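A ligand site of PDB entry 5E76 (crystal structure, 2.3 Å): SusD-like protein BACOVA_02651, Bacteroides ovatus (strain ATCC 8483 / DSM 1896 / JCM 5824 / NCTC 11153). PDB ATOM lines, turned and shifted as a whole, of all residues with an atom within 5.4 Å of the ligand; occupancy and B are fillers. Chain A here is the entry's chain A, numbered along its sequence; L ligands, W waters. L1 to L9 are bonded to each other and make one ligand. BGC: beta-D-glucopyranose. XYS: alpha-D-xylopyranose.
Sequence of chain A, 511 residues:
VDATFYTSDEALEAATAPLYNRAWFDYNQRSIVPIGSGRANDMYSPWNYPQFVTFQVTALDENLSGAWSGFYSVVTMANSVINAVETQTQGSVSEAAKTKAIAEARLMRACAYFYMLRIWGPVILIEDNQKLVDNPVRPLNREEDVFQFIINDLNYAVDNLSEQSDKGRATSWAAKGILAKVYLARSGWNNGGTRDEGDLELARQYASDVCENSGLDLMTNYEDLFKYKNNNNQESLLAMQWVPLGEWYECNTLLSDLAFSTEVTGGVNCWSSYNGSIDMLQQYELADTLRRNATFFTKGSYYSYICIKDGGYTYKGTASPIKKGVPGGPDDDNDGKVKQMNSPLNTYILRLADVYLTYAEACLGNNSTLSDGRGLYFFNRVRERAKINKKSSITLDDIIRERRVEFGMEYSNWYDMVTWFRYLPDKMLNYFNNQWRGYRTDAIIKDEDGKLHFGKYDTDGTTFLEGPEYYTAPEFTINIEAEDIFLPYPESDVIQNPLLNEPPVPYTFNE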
ATOM      1  N   GLN A  29      19.265  17.583   1.992  1.00  0.00           N
ATOM      2  CA  GLN A  29      18.401  18.751   2.093  1.00  0.00           C
ATOM      3  C   GLN A  29      18.764  19.652   3.280  1.00  0.00           C
ATOM      4  O   GLN A  29      18.669  20.879   3.190  1.00  0.00           O
ATOM      5  CB  GLN A  29      16.923  18.327   2.199  1.00  0.00           C
ATOM      6  CG  GLN A  29      15.996  19.506   2.512  1.00  0.00           C
ATOM      7  CD  GLN A  29      14.474  19.196   2.522  1.00  0.00           C
ATOM      8  OE1 GLN A  29      14.040  18.030   2.436  1.00  0.00           O
ATOM      9  NE2 GLN A  29      13.679  20.245   2.644  1.00  0.00           N
ATOM     10  N   ARG A  30      19.182  19.042   4.379  1.00  0.00           N
ATOM     11  CA  ARG A  30      19.432  19.770   5.608  1.00  0.00           C
ATOM     12  C   ARG A  30      20.216  18.965   6.661  1.00  0.00           C
ATOM     13  O   ARG A  30      21.237  19.422   7.146  1.00  0.00           O
ATOM     14  CB  ARG A  30      18.127  20.252   6.240  1.00  0.00           C
ATOM     15  CG  ARG A  30      18.261  20.615   7.719  1.00  0.00           C
ATOM     16  CD  ARG A  30      17.172  21.551   8.196  1.00  0.00           C
ATOM     17  NE  ARG A  30      17.229  22.802   7.470  1.00  0.00           N
ATOM     18  CZ  ARG A  30      16.184  23.603   7.251  1.00  0.00           C
ATOM     19  NH1 ARG A  30      14.986  23.297   7.724  1.00  0.00           N
ATOM     20  NH2 ARG A  30      16.345  24.723   6.550  1.00  0.00           N
ATOM     21  N   SER A  45      25.292  27.016  16.663  1.00  0.00           N
ATOM     22  CA  SER A  45      24.317  28.052  16.829  1.00  0.00           C
ATOM     23  C   SER A  45      23.282  27.660  17.880  1.00  0.00           C
ATOM     24  O   SER A  45      22.695  26.563  17.821  1.00  0.00           O
ATOM     25  CB  SER A  45      23.603  28.343  15.522  1.00  0.00           C
ATOM     26  OG  SER A  45      22.580  29.308  15.730  1.00  0.00           O
ATOM     27  N   TRP A  47      20.498  28.749  17.932  1.00  0.00           N
ATOM     28  CA  TRP A  47      19.210  28.927  17.282  1.00  0.00           C
ATOM     29  C   TRP A  47      19.123  28.059  16.029  1.00  0.00           C
ATOM     30  O   TRP A  47      18.085  28.025  15.378  1.00  0.00           O
ATOM     31  CB  TRP A  47      18.959  30.412  16.950  1.00  0.00           C
ATOM     32  CG  TRP A  47      19.193  31.271  18.182  1.00  0.00           C
ATOM     33  CD1 TRP A  47      18.476  31.236  19.350  1.00  0.00           C
ATOM     34  CD2 TRP A  47      20.250  32.220  18.388  1.00  0.00           C
ATOM     35  NE1 TRP A  47      19.016  32.113  20.269  1.00  0.00           N
ATOM     36  CE2 TRP A  47      20.102  32.733  19.705  1.00  0.00           C
ATOM     37  CE3 TRP A  47      21.313  32.684  17.592  1.00  0.00           C
ATOM     38  CZ2 TRP A  47      20.962  33.692  20.243  1.00  0.00           C
ATOM     39  CZ3 TRP A  47      22.169  33.653  18.121  1.00  0.00           C
ATOM     40  CH2 TRP A  47      21.996  34.148  19.440  1.00  0.00           C
ATOM     41  N   ASN A  48      20.203  27.346  15.683  1.00  0.00           N
ATOM     42  CA  ASN A  48      20.122  26.344  14.600  1.00  0.00           C
ATOM     43  C   ASN A  48      20.523  24.937  15.080  1.00  0.00           C
ATOM     44  O   ASN A  48      21.633  24.482  14.821  1.00  0.00           O
ATOM     45  CB  ASN A  48      20.983  26.737  13.401  1.00  0.00           C
ATOM     46  CG  ASN A  48      20.415  27.907  12.601  1.00  0.00           C
ATOM     47  OD1 ASN A  48      19.337  28.424  12.931  1.00  0.00           O
ATOM     48  ND2 ASN A  48      21.147  28.338  11.564  1.00  0.00           N
ATOM     49  N   TYR A  49      19.595  24.253  15.759  1.00  0.00           N
ATOM     50  CA  TYR A  49      19.778  22.870  16.128  1.00  0.00           C
ATOM     51  C   TYR A  49      20.977  22.619  17.008  1.00  0.00           C
ATOM     52  O   TYR A  49      21.787  21.765  16.687  1.00  0.00           O
ATOM     53  CB  TYR A  49      19.927  22.016  14.875  1.00  0.00           C
ATOM     54  CG  TYR A  49      18.765  22.109  13.917  1.00  0.00           C
ATOM     55  CD1 TYR A  49      17.509  21.682  14.307  1.00  0.00           C
ATOM     56  CD2 TYR A  49      18.922  22.619  12.631  1.00  0.00           C
ATOM     57  CE1 TYR A  49      16.453  21.748  13.474  1.00  0.00           C
ATOM     58  CE2 TYR A  49      17.843  22.714  11.763  1.00  0.00           C
ATOM     59  CZ  TYR A  49      16.599  22.264  12.200  1.00  0.00           C
ATOM     60  OH  TYR A  49      15.495  22.324  11.393  1.00  0.00           O
ATOM     61  N   GLU A  62      13.571  16.244  13.918  1.00  0.00           N
ATOM     62  CA  GLU A  62      13.247  16.197  12.501  1.00  0.00           C
ATOM     63  C   GLU A  62      14.471  15.868  11.629  1.00  0.00           C
ATOM     64  O   GLU A  62      14.325  15.242  10.576  1.00  0.00           O
ATOM     65  CB  GLU A  62      12.630  17.538  12.076  1.00  0.00           C
ATOM     66  CG  GLU A  62      13.570  18.705  12.376  1.00  0.00           C
ATOM     67  CD  GLU A  62      13.012  20.038  11.891  1.00  0.00           C
ATOM     68  OE1 GLU A  62      13.783  20.817  11.272  1.00  0.00           O
ATOM     69  OE2 GLU A  62      11.813  20.292  12.136  1.00  0.00           O
ATOM     70  N   TRP A 248      13.378  20.850  -7.472  1.00  0.00           N
ATOM     71  CA  TRP A 248      13.324  20.162  -6.204  1.00  0.00           C
ATOM     72  C   TRP A 248      13.634  18.695  -6.415  1.00  0.00           C
ATOM     73  O   TRP A 248      13.360  18.140  -7.486  1.00  0.00           O
ATOM     74  CB  TRP A 248      11.947  20.310  -5.579  1.00  0.00           C
ATOM     75  CG  TRP A 248      11.917  20.126  -4.091  1.00  0.00           C
ATOM     76  CD1 TRP A 248      11.420  19.048  -3.392  1.00  0.00           C
ATOM     77  CD2 TRP A 248      12.409  21.045  -3.112  1.00  0.00           C
ATOM     78  NE1 TRP A 248      11.574  19.255  -2.049  1.00  0.00           N
ATOM     79  CE2 TRP A 248      12.174  20.473  -1.840  1.00  0.00           C
ATOM     80  CE3 TRP A 248      13.028  22.303  -3.196  1.00  0.00           C
ATOM     81  CZ2 TRP A 248      12.527  21.121  -0.662  1.00  0.00           C
ATOM     82  CZ3 TRP A 248      13.382  22.942  -2.028  1.00  0.00           C
ATOM     83  CH2 TRP A 248      13.123  22.344  -0.766  1.00  0.00           C
ATOM     84  N   TYR A 249      14.174  18.073  -5.364  1.00  0.00           N
ATOM     85  CA  TYR A 249      14.588  16.670  -5.332  1.00  0.00           C
ATOM     86  C   TYR A 249      15.896  16.462  -6.063  1.00  0.00           C
ATOM     87  O   TYR A 249      16.429  15.356  -6.053  1.00  0.00           O
ATOM     88  CB  TYR A 249      13.533  15.714  -5.913  1.00  0.00           C
ATOM     89  CG  TYR A 249      12.263  15.640  -5.098  1.00  0.00           C
ATOM     90  CD1 TYR A 249      11.161  16.385  -5.424  1.00  0.00           C
ATOM     91  CD2 TYR A 249      12.189  14.818  -3.980  1.00  0.00           C
ATOM     92  CE1 TYR A 249       9.999  16.316  -4.664  1.00  0.00           C
ATOM     93  CE2 TYR A 249      11.053  14.735  -3.214  1.00  0.00           C
ATOM     94  CZ  TYR A 249       9.968  15.486  -3.552  1.00  0.00           C
ATOM     95  OH  TYR A 249       8.845  15.396  -2.779  1.00  0.00           O
ATOM     96  N   ASP A 257      20.859  27.804   4.473  1.00  0.00           N
ATOM     97  CA  ASP A 257      21.236  27.272   5.786  1.00  0.00           C
ATOM     98  C   ASP A 257      22.729  27.564   6.122  1.00  0.00           C
ATOM     99  O   ASP A 257      23.079  27.679   7.299  1.00  0.00           O
ATOM    100  CB  ASP A 257      21.019  25.749   5.875  1.00  0.00           C
ATOM    101  CG  ASP A 257      19.562  25.322   5.877  1.00  0.00           C
ATOM    102  OD1 ASP A 257      18.640  26.183   5.880  1.00  0.00           O
ATOM    103  OD2 ASP A 257      19.323  24.096   5.881  1.00  0.00           O
ATOM    104  N   ASN A 269      18.415  35.187  -0.612  1.00  0.00           N
ATOM    105  CA  ASN A 269      17.923  35.033   0.759  1.00  0.00           C
ATOM    106  C   ASN A 269      18.656  33.925   1.511  1.00  0.00           C
ATOM    107  O   ASN A 269      18.953  32.864   0.939  1.00  0.00           O
ATOM    108  CB  ASN A 269      16.412  34.750   0.749  1.00  0.00           C
ATOM    109  CG  ASN A 269      15.813  34.720   2.145  1.00  0.00           C
ATOM    110  OD1 ASN A 269      16.175  35.534   3.002  1.00  0.00           O
ATOM    111  ND2 ASN A 269      14.877  33.816   2.372  1.00  0.00           N
ATOM    112  N   TRP A 271      19.880  32.761   6.009  1.00  0.00           N
ATOM    113  CA  TRP A 271      19.552  32.953   7.405  1.00  0.00           C
ATOM    114  C   TRP A 271      20.457  32.242   8.389  1.00  0.00           C
ATOM    115  O   TRP A 271      20.177  32.262   9.583  1.00  0.00           O
ATOM    116  CB  TRP A 271      18.101  32.489   7.647  1.00  0.00           C
ATOM    117  CG  TRP A 271      17.881  31.133   7.112  1.00  0.00           C
ATOM    118  CD1 TRP A 271      18.410  29.970   7.593  1.00  0.00           C
ATOM    119  CD2 TRP A 271      17.112  30.774   5.962  1.00  0.00           C
ATOM    120  NE1 TRP A 271      18.011  28.917   6.814  1.00  0.00           N
ATOM    121  CE2 TRP A 271      17.208  29.377   5.806  1.00  0.00           C
ATOM    122  CE3 TRP A 271      16.325  31.499   5.045  1.00  0.00           C
ATOM    123  CZ2 TRP A 271      16.550  28.688   4.787  1.00  0.00           C
ATOM    124  CZ3 TRP A 271      15.688  30.815   4.034  1.00  0.00           C
ATOM    125  CH2 TRP A 271      15.805  29.431   3.906  1.00  0.00           C
ATOM    126  N   SER A 272      21.508  31.586   7.930  1.00  0.00           N
ATOM    127  CA  SER A 272      22.432  30.889   8.841  1.00  0.00           C
ATOM    128  C   SER A 272      22.887  31.731  10.031  1.00  0.00           C
ATOM    129  O   SER A 272      23.293  32.865   9.875  1.00  0.00           O
ATOM    130  CB  SER A 272      23.679  30.392   8.114  1.00  0.00           C
ATOM    131  OG  SER A 272      24.291  29.343   8.878  1.00  0.00           O
ATOM    132  N   SER A 273      22.802  31.149  11.211  1.00  0.00           N
ATOM    133  CA  SER A 273      23.332  31.770  12.414  1.00  0.00           C
ATOM    134  C   SER A 273      24.461  30.920  12.981  1.00  0.00           C
ATOM    135  O   SER A 273      24.863  31.072  14.143  1.00  0.00           O
ATOM    136  CB  SER A 273      22.214  31.935  13.420  1.00  0.00           C
ATOM    137  OG  SER A 273      21.536  30.693  13.493  1.00  0.00           O
ATOM    138  N   GLN A 340      18.068  30.982  -3.415  1.00  0.00           N
ATOM    139  CA  GLN A 340      17.798  30.446  -2.085  1.00  0.00           C
ATOM    140  C   GLN A 340      17.524  28.949  -2.169  1.00  0.00           C
ATOM    141  O   GLN A 340      16.875  28.472  -3.111  1.00  0.00           O
ATOM    142  CB  GLN A 340      16.625  31.169  -1.421  1.00  0.00           C
ATOM    143  CG  GLN A 340      15.226  30.688  -1.786  1.00  0.00           C
ATOM    144  CD  GLN A 340      14.219  31.130  -0.742  1.00  0.00           C
ATOM    145  OE1 GLN A 340      14.333  32.213  -0.184  1.00  0.00           O
ATOM    146  NE2 GLN A 340      13.211  30.274  -0.472  1.00  0.00           N
ATOM    147  N   MET A 341      18.057  28.218  -1.187  1.00  0.00           N
ATOM    148  CA  MET A 341      17.957  26.768  -1.179  1.00  0.00           C
ATOM    149  C   MET A 341      18.320  26.143  -2.544  1.00  0.00           C
ATOM    150  O   MET A 341      17.711  25.158  -2.976  1.00  0.00           O
ATOM    151  CB  MET A 341      16.548  26.329  -0.779  1.00  0.00           C
ATOM    152  CG  MET A 341      16.067  26.817   0.581  1.00  0.00           C
ATOM    153  SD  MET A 341      14.475  26.034   1.069  1.00  0.00           S
ATOM    154  CE  MET A 341      15.038  24.367   1.384  1.00  0.00           C
HETATM  155  C2  BGC L   1       7.831  19.824  -3.386  1.00  0.00           C
HETATM  156  C3  BGC L   1       7.690  20.828  -2.314  1.00  0.00           C
HETATM  157  C4  BGC L   1       8.574  21.956  -2.526  1.00  0.00           C
HETATM  158  C5  BGC L   1       8.277  22.573  -3.843  1.00  0.00           C
HETATM  159  C6  BGC L   1       9.172  23.735  -4.144  1.00  0.00           C
HETATM  160  C1  BGC L   1       7.569  20.390  -4.804  1.00  0.00           C
HETATM  161  O1  BGC L   1       7.922  19.517  -5.692  1.00  0.00           O
HETATM  162  O2  BGC L   1       6.923  18.766  -3.115  1.00  0.00           O
HETATM  163  O3  BGC L   1       7.956  20.204  -1.014  1.00  0.00           O
HETATM  164  O4  BGC L   1       8.367  22.916  -1.418  1.00  0.00           O
HETATM  165  O5  BGC L   1       8.442  21.644  -4.963  1.00  0.00           O
HETATM  166  O6  BGC L   1       9.172  23.952  -5.534  1.00  0.00           O
HETATM  167  C2  BGC L   2       9.380  24.660  -0.089  1.00  0.00           C
HETATM  168  C3  BGC L   2      10.433  25.081   0.855  1.00  0.00           C
HETATM  169  C4  BGC L   2      10.470  24.365   2.128  1.00  0.00           C
HETATM  170  C5  BGC L   2      10.378  22.896   1.972  1.00  0.00           C
HETATM  171  C6  BGC L   2      10.246  22.218   3.322  1.00  0.00           C
HETATM  172  C1  BGC L   2       9.253  23.129  -0.256  1.00  0.00           C
HETATM  173  O2  BGC L   2       9.716  25.215  -1.345  1.00  0.00           O
HETATM  174  O3  BGC L   2      10.223  26.515   1.131  1.00  0.00           O
HETATM  175  O4  BGC L   2      11.734  24.735   2.766  1.00  0.00           O
HETATM  176  O5  BGC L   2       9.200  22.528   1.161  1.00  0.00           O
HETATM  177  O6  BGC L   2      10.147  20.834   3.133  1.00  0.00           O
HETATM  178  C2  BGC L   3      12.679  25.485   5.006  1.00  0.00           C
HETATM  179  C3  BGC L   3      12.420  26.490   6.053  1.00  0.00           C
HETATM  180  C4  BGC L   3      12.416  27.823   5.463  1.00  0.00           C
HETATM  181  C5  BGC L   3      11.357  27.899   4.449  1.00  0.00           C
HETATM  182  C6  BGC L   3      11.200  29.317   3.937  1.00  0.00           C
HETATM  183  C1  BGC L   3      11.569  25.534   3.926  1.00  0.00           C
HETATM  184  O2  BGC L   3      12.745  24.199   5.612  1.00  0.00           O
HETATM  185  O3  BGC L   3      13.426  26.362   7.111  1.00  0.00           O
HETATM  186  O4  BGC L   3      12.141  28.837   6.484  1.00  0.00           O
HETATM  187  O5  BGC L   3      11.668  26.954   3.369  1.00  0.00           O
HETATM  188  O6  BGC L   3      10.875  29.294   2.572  1.00  0.00           O
HETATM  189  C2  BGC L   4      12.604  30.709   7.817  1.00  0.00           C
HETATM  190  C3  BGC L   4      13.644  31.478   8.618  1.00  0.00           C
HETATM  191  C4  BGC L   4      14.347  30.564   9.613  1.00  0.00           C
HETATM  192  C5  BGC L   4      14.833  29.285   8.937  1.00  0.00           C
HETATM  193  C6  BGC L   4      15.474  28.340   9.948  1.00  0.00           C
HETATM  194  C1  BGC L   4      13.190  29.415   7.248  1.00  0.00           C
HETATM  195  O2  BGC L   4      12.119  31.527   6.744  1.00  0.00           O
HETATM  196  O3  BGC L   4      13.000  32.553   9.319  1.00  0.00           O
HETATM  197  O4  BGC L   4      15.467  31.257  10.184  1.00  0.00           O
HETATM  198  O5  BGC L   4      13.735  28.636   8.305  1.00  0.00           O
HETATM  199  O6  BGC L   4      15.268  26.983   9.542  1.00  0.00           O
HETATM  200  C1  XYS L   5      10.194  30.171   1.592  1.00  0.00           C
HETATM  201  C2  XYS L   5      10.569  31.622   1.607  1.00  0.00           C
HETATM  202  C3  XYS L   5       9.692  32.283   2.691  1.00  0.00           C
HETATM  203  C4  XYS L   5       8.207  32.084   2.300  1.00  0.00           C
HETATM  204  C5  XYS L   5       7.982  30.559   2.208  1.00  0.00           C
HETATM  205  O2  XYS L   5      11.878  31.700   2.083  1.00  0.00           O
HETATM  206  O3  XYS L   5       9.919  33.662   2.610  1.00  0.00           O
HETATM  207  O4  XYS L   5       7.436  32.524   3.383  1.00  0.00           O
HETATM  208  O5  XYS L   5       8.891  30.073   1.215  1.00  0.00           O
HETATM  209  C2  BGC L   6      17.304  31.538  11.597  1.00  0.00           C
HETATM  210  C3  BGC L   6      17.495  31.594  13.064  1.00  0.00           C
HETATM  211  C4  BGC L   6      16.626  32.610  13.649  1.00  0.00           C
HETATM  212  C5  BGC L   6      15.204  32.351  13.376  1.00  0.00           C
HETATM  213  C6  BGC L   6      14.402  33.515  13.924  1.00  0.00           C
HETATM  214  C1  BGC L   6      15.850  31.127  11.296  1.00  0.00           C
HETATM  215  O2  BGC L   6      18.223  30.632  10.993  1.00  0.00           O
HETATM  216  O3  BGC L   6      18.916  31.870  13.368  1.00  0.00           O
HETATM  217  O4  BGC L   6      16.791  32.640  15.097  1.00  0.00           O
HETATM  218  O5  BGC L   6      14.969  32.205  11.939  1.00  0.00           O
HETATM  219  O6  BGC L   6      13.217  33.701  13.189  1.00  0.00           O
HETATM  220  C1  XYS L   7      15.277  25.625   9.918  1.00  0.00           C
HETATM  221  C2  XYS L   7      13.986  25.022  10.470  1.00  0.00           C
HETATM  222  C3  XYS L   7      13.630  25.643  11.804  1.00  0.00           C
HETATM  223  C4  XYS L   7      14.827  25.644  12.755  1.00  0.00           C
HETATM  224  C5  XYS L   7      16.063  26.205  12.064  1.00  0.00           C
HETATM  225  O2  XYS L   7      12.928  25.236   9.538  1.00  0.00           O
HETATM  226  O3  XYS L   7      12.550  24.906  12.398  1.00  0.00           O
HETATM  227  O4  XYS L   7      14.518  26.433  13.913  1.00  0.00           O
HETATM  228  O5  XYS L   7      16.322  25.468  10.876  1.00  0.00           O
HETATM  229  C2  BGC L   8      16.933  33.968  17.098  1.00  0.00           C
HETATM  230  C3  BGC L   8      17.419  35.208  17.740  1.00  0.00           C
HETATM  231  C4  BGC L   8      18.832  35.498  17.459  1.00  0.00           C
HETATM  232  C5  BGC L   8      19.053  35.504  15.992  1.00  0.00           C
HETATM  233  C6  BGC L   8      20.427  36.020  15.573  1.00  0.00           C
HETATM  234  C1  BGC L   8      17.393  33.767  15.642  1.00  0.00           C
HETATM  235  O2  BGC L   8      15.517  33.996  17.061  1.00  0.00           O
HETATM  236  O3  BGC L   8      17.171  35.072  19.180  1.00  0.00           O
HETATM  237  O4  BGC L   8      19.210  36.799  18.039  1.00  0.00           O
HETATM  238  O5  BGC L   8      18.876  34.132  15.520  1.00  0.00           O
HETATM  239  O6  BGC L   8      20.514  36.035  14.155  1.00  0.00           O
HETATM  240  C2  BGC L   9      20.592  38.597  19.241  1.00  0.00           C
HETATM  241  C3  BGC L   9      21.209  38.863  20.566  1.00  0.00           C
HETATM  242  C4  BGC L   9      20.261  38.729  21.666  1.00  0.00           C
HETATM  243  C5  BGC L   9      19.636  37.386  21.663  1.00  0.00           C
HETATM  244  C6  BGC L   9      18.654  37.279  22.811  1.00  0.00           C
HETATM  245  C1  BGC L   9      19.933  37.208  19.189  1.00  0.00           C
HETATM  246  O2  BGC L   9      21.594  38.684  18.221  1.00  0.00           O
HETATM  247  O3  BGC L   9      21.756  40.233  20.602  1.00  0.00           O
HETATM  248  O4  BGC L   9      20.964  38.930  22.943  1.00  0.00           O
HETATM  249  O5  BGC L   9      18.971  37.090  20.393  1.00  0.00           O
HETATM  250  O6  BGC L   9      17.664  36.319  22.504  1.00  0.00           O
HETATM  251  O   HOH W   1      10.149  34.600   4.841  1.00  0.00           O
HETATM  252  O   HOH W   2      13.131  22.615  14.229  1.00  0.00           O
HETATM  253  O   HOH W   3      14.713  22.063   4.624  1.00  0.00           O
HETATM  254  O   HOH W   4      14.759  31.065  17.444  1.00  0.00           O
HETATM  255  O   HOH W   5      11.840  35.681  13.344  1.00  0.00           O
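OG of Ser 273 lies within hydrogen-bond range of O3 of BGC L6, at 2.9 Å. O of Trp 271 sits at hydrogen-bond distance from O2 of BGC L6, 2.9 Å away. The side-chain amide oxygen of Asn 48 is in hydrogen-bond range of an oxygen (O2) of BGC L6, at 3.1 Å. The guanidinium group of Arg 30 sits at hydrogen-bond distance from an oxygen (O2) of BGC L3, 3.2 Å away. NE2 of Gln 340 sits at hydrogen-bond distance from O2 of XYS L5, at 3.2 Å. OH of Tyr 49 lies close to O5 of XYS L7 (3.3 Å).
The side-chain amide nitrogen (ND2) of Asn 48 lies within hydrogen-bond range of the side-chain hydroxyl (OG) of Ser 273 (3.1 Å). OG of Ser 45 lies within hydrogen-bond range of OG of Ser 273 (2.8 Å). The indole nitrogen (NE1) of Trp 271 lies within hydrogen-bond range of the side-chain carboxylate (OD1) of Asp 257 (3.0 Å). The backbone NH (N) of Asn 48 lies within hydrogen-bond range of the side-chain hydroxyl (OG) of Ser 45 (3.1 Å). The guanidinium group (NH2) of Arg 30 lies within salt-bridge range of the side-chain carboxylate (OD1) of Asp 257 (2.8 Å). The side-chain amide nitrogen (ND2) of Asn 269 lies within hydrogen-bond range of the side-chain amide oxygen (OE1) of Gln 340 (3.1 Å). N of Trp 47 lies close to OG of Ser 45 (3.1 Å).
O4 of BGC L2 lies close to SD of Met 341. Merely in contact with the ligand: Trp 47, Gln 29, Trp 248, Asn 269 and Tyr 249. Hydrophobic or aromatic side chains that line the ligand: Trp 47, Tyr 49, Trp 248, Tyr 249, Trp 271 and Met 341. Within 4 Å of the ligand: Gln 29, Arg 30, Trp 47, Asn 48, Tyr 49, Trp 248, Tyr 249, Asn 269, Trp 271, Ser 273, Gln 340 and Met 341. The nearest printed residue that does not touch the ligand is Glu 62 (4.3 Å).
Water W2 lies within hydrogen-bond range of O3 of XYS L7 (3.0 Å) and OE2 of Glu 62 (3.4 Å). Water W3 lies within hydrogen-bond range of NE2 of Gln 29 (2.9 Å), O2 of BGC L3 (3.1 Å) and NH1 of Arg 30 (3.3 Å).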
